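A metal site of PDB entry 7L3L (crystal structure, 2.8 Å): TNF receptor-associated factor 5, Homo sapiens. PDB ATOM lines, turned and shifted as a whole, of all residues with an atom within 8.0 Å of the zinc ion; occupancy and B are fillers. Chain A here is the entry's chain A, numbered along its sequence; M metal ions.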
ATOM      1  N   LYS A  22     -11.571  19.998   3.209  1.00  0.00           N
ATOM      2  CA  LYS A  22     -11.817  18.607   3.566  1.00  0.00           C
ATOM      3  C   LYS A  22     -11.450  18.384   5.026  1.00  0.00           C
ATOM      4  O   LYS A  22     -10.516  18.992   5.558  1.00  0.00           O
ATOM      5  CB  LYS A  22     -10.997  17.670   2.674  1.00  0.00           C
ATOM      6  CG  LYS A  22     -11.499  17.559   1.237  1.00  0.00           C
ATOM      7  CD  LYS A  22     -10.575  16.688   0.390  1.00  0.00           C
ATOM      8  CE  LYS A  22     -10.966  16.707  -1.072  1.00  0.00           C
ATOM      9  NZ  LYS A  22      -9.923  16.077  -1.939  1.00  0.00           N
ATOM     10  N   CYS A  23     -12.209  17.502   5.680  1.00  0.00           N
ATOM     11  CA  CYS A  23     -11.980  17.175   7.073  1.00  0.00           C
ATOM     12  C   CYS A  23     -10.662  16.424   7.243  1.00  0.00           C
ATOM     13  O   CYS A  23     -10.264  15.632   6.388  1.00  0.00           O
ATOM     14  CB  CYS A  23     -13.137  16.345   7.619  1.00  0.00           C
ATOM     15  SG  CYS A  23     -12.773  15.383   9.104  1.00  0.00           S
ATOM     16  N   ALA A  24      -9.985  16.679   8.363  1.00  0.00           N
ATOM     17  CA  ALA A  24      -8.694  16.052   8.615  1.00  0.00           C
ATOM     18  C   ALA A  24      -8.811  14.606   9.101  1.00  0.00           C
ATOM     19  O   ALA A  24      -7.780  13.954   9.277  1.00  0.00           O
ATOM     20  CB  ALA A  24      -7.894  16.865   9.630  1.00  0.00           C
ATOM     21  N   PHE A  25     -10.027  14.111   9.329  1.00  0.00           N
ATOM     22  CA  PHE A  25     -10.237  12.741   9.755  1.00  0.00           C
ATOM     23  C   PHE A  25     -11.060  11.929   8.770  1.00  0.00           C
ATOM     24  O   PHE A  25     -10.621  10.861   8.343  1.00  0.00           O
ATOM     25  CB  PHE A  25     -10.908  12.714  11.140  1.00  0.00           C
ATOM     26  CG  PHE A  25     -11.218  11.336  11.635  1.00  0.00           C
ATOM     27  CD1 PHE A  25     -10.240  10.554  12.220  1.00  0.00           C
ATOM     28  CD2 PHE A  25     -12.498  10.813  11.522  1.00  0.00           C
ATOM     29  CE1 PHE A  25     -10.523   9.276  12.673  1.00  0.00           C
ATOM     30  CE2 PHE A  25     -12.795   9.539  11.975  1.00  0.00           C
ATOM     31  CZ  PHE A  25     -11.797   8.769  12.557  1.00  0.00           C
ATOM     32  N   CYS A  26     -12.242  12.407   8.396  1.00  0.00           N
ATOM     33  CA  CYS A  26     -13.099  11.676   7.472  1.00  0.00           C
ATOM     34  C   CYS A  26     -12.772  11.941   6.012  1.00  0.00           C
ATOM     35  O   CYS A  26     -13.199  11.180   5.146  1.00  0.00           O
ATOM     36  CB  CYS A  26     -14.575  12.028   7.733  1.00  0.00           C
ATOM     37  SG  CYS A  26     -15.162  13.465   6.810  1.00  0.00           S
ATOM     38  N   HIS A  27     -12.041  13.028   5.736  1.00  0.00           N
ATOM     39  CA  HIS A  27     -11.569  13.446   4.420  1.00  0.00           C
ATOM     40  C   HIS A  27     -12.711  13.901   3.504  1.00  0.00           C
ATOM     41  O   HIS A  27     -12.434  14.350   2.378  1.00  0.00           O
ATOM     42  CB  HIS A  27     -10.757  12.361   3.706  1.00  0.00           C
ATOM     43  CG  HIS A  27      -9.564  11.894   4.493  1.00  0.00           C
ATOM     44  ND1 HIS A  27      -8.576  12.743   4.927  1.00  0.00           N
ATOM     45  CD2 HIS A  27      -9.206  10.655   4.903  1.00  0.00           C
ATOM     46  CE1 HIS A  27      -7.654  12.062   5.579  1.00  0.00           C
ATOM     47  NE2 HIS A  27      -8.010  10.787   5.583  1.00  0.00           N
ATOM     48  N   SER A  28     -13.959  13.811   3.933  1.00  0.00           N
ATOM     49  CA  SER A  28     -15.058  14.336   3.131  1.00  0.00           C
ATOM     50  C   SER A  28     -15.098  15.859   3.257  1.00  0.00           C
ATOM     51  O   SER A  28     -14.284  16.474   3.959  1.00  0.00           O
ATOM     52  CB  SER A  28     -16.387  13.718   3.574  1.00  0.00           C
ATOM     53  OG  SER A  28     -16.335  12.302   3.540  1.00  0.00           O
ATOM     54  N   VAL A  29     -16.058  16.471   2.569  1.00  0.00           N
ATOM     55  CA  VAL A  29     -16.231  17.909   2.692  1.00  0.00           C
ATOM     56  C   VAL A  29     -16.783  18.234   4.081  1.00  0.00           C
ATOM     57  O   VAL A  29     -17.623  17.499   4.620  1.00  0.00           O
ATOM     58  CB  VAL A  29     -17.136  18.458   1.569  1.00  0.00           C
ATOM     59  CG1 VAL A  29     -18.596  18.107   1.819  1.00  0.00           C
ATOM     60  CG2 VAL A  29     -16.955  19.957   1.424  1.00  0.00           C
ATOM     61  N   LEU A  30     -16.284  19.322   4.659  1.00  0.00           N
ATOM     62  CA  LEU A  30     -16.613  19.644   6.039  1.00  0.00           C
ATOM     63  C   LEU A  30     -18.107  19.892   6.187  1.00  0.00           C
ATOM     64  O   LEU A  30     -18.709  20.675   5.444  1.00  0.00           O
ATOM     65  CB  LEU A  30     -15.832  20.876   6.482  1.00  0.00           C
ATOM     66  CG  LEU A  30     -14.358  20.616   6.799  1.00  0.00           C
ATOM     67  CD1 LEU A  30     -13.558  21.894   6.672  1.00  0.00           C
ATOM     68  CD2 LEU A  30     -14.222  20.036   8.189  1.00  0.00           C
ATOM     69  N   HIS A  31     -18.720  19.215   7.150  1.00  0.00           N
ATOM     70  CA  HIS A  31     -20.101  19.480   7.544  1.00  0.00           C
ATOM     71  C   HIS A  31     -20.105  19.991   8.970  1.00  0.00           C
ATOM     72  O   HIS A  31     -19.666  19.286   9.884  1.00  0.00           O
ATOM     73  CB  HIS A  31     -20.962  18.227   7.419  1.00  0.00           C
ATOM     74  CG  HIS A  31     -22.391  18.462   7.825  1.00  0.00           C
ATOM     75  ND1 HIS A  31     -22.998  17.740   8.825  1.00  0.00           N
ATOM     76  CD2 HIS A  31     -23.307  19.351   7.383  1.00  0.00           C
ATOM     77  CE1 HIS A  31     -24.246  18.164   8.967  1.00  0.00           C
ATOM     78  NE2 HIS A  31     -24.453  19.136   8.105  1.00  0.00           N
ATOM     79  N   ARG A  41      -9.369  21.340  10.877  1.00  0.00           N
ATOM     80  CA  ARG A  41     -10.823  21.362  10.770  1.00  0.00           C
ATOM     81  C   ARG A  41     -11.373  19.948  10.683  1.00  0.00           C
ATOM     82  O   ARG A  41     -10.784  19.072  10.043  1.00  0.00           O
ATOM     83  CB  ARG A  41     -11.260  22.163   9.535  1.00  0.00           C
ATOM     84  CG  ARG A  41     -10.788  23.606   9.545  1.00  0.00           C
ATOM     85  CD  ARG A  41     -10.859  24.221   8.157  1.00  0.00           C
ATOM     86  NE  ARG A  41     -11.003  25.677   8.205  1.00  0.00           N
ATOM     87  CZ  ARG A  41     -10.753  26.492   7.186  1.00  0.00           C
ATOM     88  NH1 ARG A  41     -10.353  25.997   6.018  1.00  0.00           N
ATOM     89  NH2 ARG A  41     -10.905  27.795   7.320  1.00  0.00           N
ATOM     90  N   PHE A  42     -12.514  19.724  11.336  1.00  0.00           N
ATOM     91  CA  PHE A  42     -13.180  18.439  11.317  1.00  0.00           C
ATOM     92  C   PHE A  42     -14.672  18.658  11.233  1.00  0.00           C
ATOM     93  O   PHE A  42     -15.182  19.692  11.679  1.00  0.00           O
ATOM     94  CB  PHE A  42     -12.873  17.605  12.573  1.00  0.00           C
ATOM     95  CG  PHE A  42     -11.410  17.493  12.896  1.00  0.00           C
ATOM     96  CD1 PHE A  42     -10.769  18.481  13.619  1.00  0.00           C
ATOM     97  CD2 PHE A  42     -10.684  16.391  12.479  1.00  0.00           C
ATOM     98  CE1 PHE A  42      -9.427  18.380  13.916  1.00  0.00           C
ATOM     99  CE2 PHE A  42      -9.343  16.290  12.776  1.00  0.00           C
ATOM    100  CZ  PHE A  42      -8.710  17.275  13.496  1.00  0.00           C
ATOM    101  N   CYS A  43     -15.386  17.683  10.669  1.00  0.00           N
ATOM    102  CA  CYS A  43     -16.827  17.668  10.801  1.00  0.00           C
ATOM    103  C   CYS A  43     -17.202  17.658  12.274  1.00  0.00           C
ATOM    104  O   CYS A  43     -16.394  17.315  13.150  1.00  0.00           O
ATOM    105  CB  CYS A  43     -17.428  16.446  10.095  1.00  0.00           C
ATOM    106  SG  CYS A  43     -16.844  16.155   8.407  1.00  0.00           S
ATOM    107  N   GLN A  44     -18.438  18.059  12.573  1.00  0.00           N
ATOM    108  CA  GLN A  44     -18.856  18.073  13.973  1.00  0.00           C
ATOM    109  C   GLN A  44     -18.982  16.670  14.531  1.00  0.00           C
ATOM    110  O   GLN A  44     -18.573  16.399  15.669  1.00  0.00           O
ATOM    111  CB  GLN A  44     -20.165  18.827  14.135  1.00  0.00           C
ATOM    112  CG  GLN A  44     -20.545  18.975  15.587  1.00  0.00           C
ATOM    113  CD  GLN A  44     -22.005  19.285  15.789  1.00  0.00           C
ATOM    114  OE1 GLN A  44     -22.360  20.398  16.183  1.00  0.00           O
ATOM    115  NE2 GLN A  44     -22.852  18.307  15.509  1.00  0.00           N
ATOM    116  N   HIS A  45     -19.555  15.748  13.759  1.00  0.00           N
ATOM    117  CA  HIS A  45     -19.709  14.368  14.201  1.00  0.00           C
ATOM    118  C   HIS A  45     -18.396  13.614  14.226  1.00  0.00           C
ATOM    119  O   HIS A  45     -18.333  12.531  14.819  1.00  0.00           O
ATOM    120  CB  HIS A  45     -20.719  13.646  13.311  1.00  0.00           C
ATOM    121  CG  HIS A  45     -20.410  13.749  11.845  1.00  0.00           C
ATOM    122  ND1 HIS A  45     -20.636  14.895  11.109  1.00  0.00           N
ATOM    123  CD2 HIS A  45     -19.903  12.838  10.990  1.00  0.00           C
ATOM    124  CE1 HIS A  45     -20.273  14.681   9.857  1.00  0.00           C
ATOM    125  NE2 HIS A  45     -19.830  13.447   9.756  1.00  0.00           N
ATOM    126  N   CYS A  46     -17.347  14.143  13.579  1.00  0.00           N
ATOM    127  CA  CYS A  46     -16.021  13.540  13.604  1.00  0.00           C
ATOM    128  C   CYS A  46     -15.162  14.027  14.764  1.00  0.00           C
ATOM    129  O   CYS A  46     -14.213  13.344  15.145  1.00  0.00           O
ATOM    130  CB  CYS A  46     -15.274  13.799  12.297  1.00  0.00           C
ATOM    131  SG  CYS A  46     -16.105  13.220  10.816  1.00  0.00           S
ATOM    132  N   ILE A  47     -15.465  15.195  15.333  1.00  0.00           N
ATOM    133  CA  ILE A  47     -14.784  15.623  16.550  1.00  0.00           C
ATOM    134  C   ILE A  47     -15.275  14.810  17.728  1.00  0.00           C
ATOM    135  O   ILE A  47     -14.479  14.295  18.529  1.00  0.00           O
ATOM    136  CB  ILE A  47     -14.974  17.129  16.797  1.00  0.00           C
ATOM    137  CG1 ILE A  47     -14.286  17.932  15.691  1.00  0.00           C
ATOM    138  CG2 ILE A  47     -14.440  17.507  18.167  1.00  0.00           C
ATOM    139  CD1 ILE A  47     -13.864  19.314  16.118  1.00  0.00           C
HETATM  140 ZN    ZN M   1     -14.966  14.667   8.826  1.00  0.00          ZN
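The backbone NH of Phe 25 sits close to the side-chain sulfur of Cys 23. O of Ser 28 sits at hydrogen-bond distance from N of Cys 23 (2.9 Å). The backbone NH of Ser 28 lies close to the side-chain sulfur of Cys 26 (3.1 Å).
The nearest printed residue that does not touch the zinc ion is His 27 (4.6 Å).
The zinc ion is bound by the side-chain sulfur of Cys 23 (2.3 Å), the side-chain sulfur of Cys 26 (2.4 Å), the side-chain sulfur of Cys 43 (2.4 Å) and the side-chain sulfur of Cys 46 (2.7 Å). The zinc ion has four donor atoms within binding distance.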
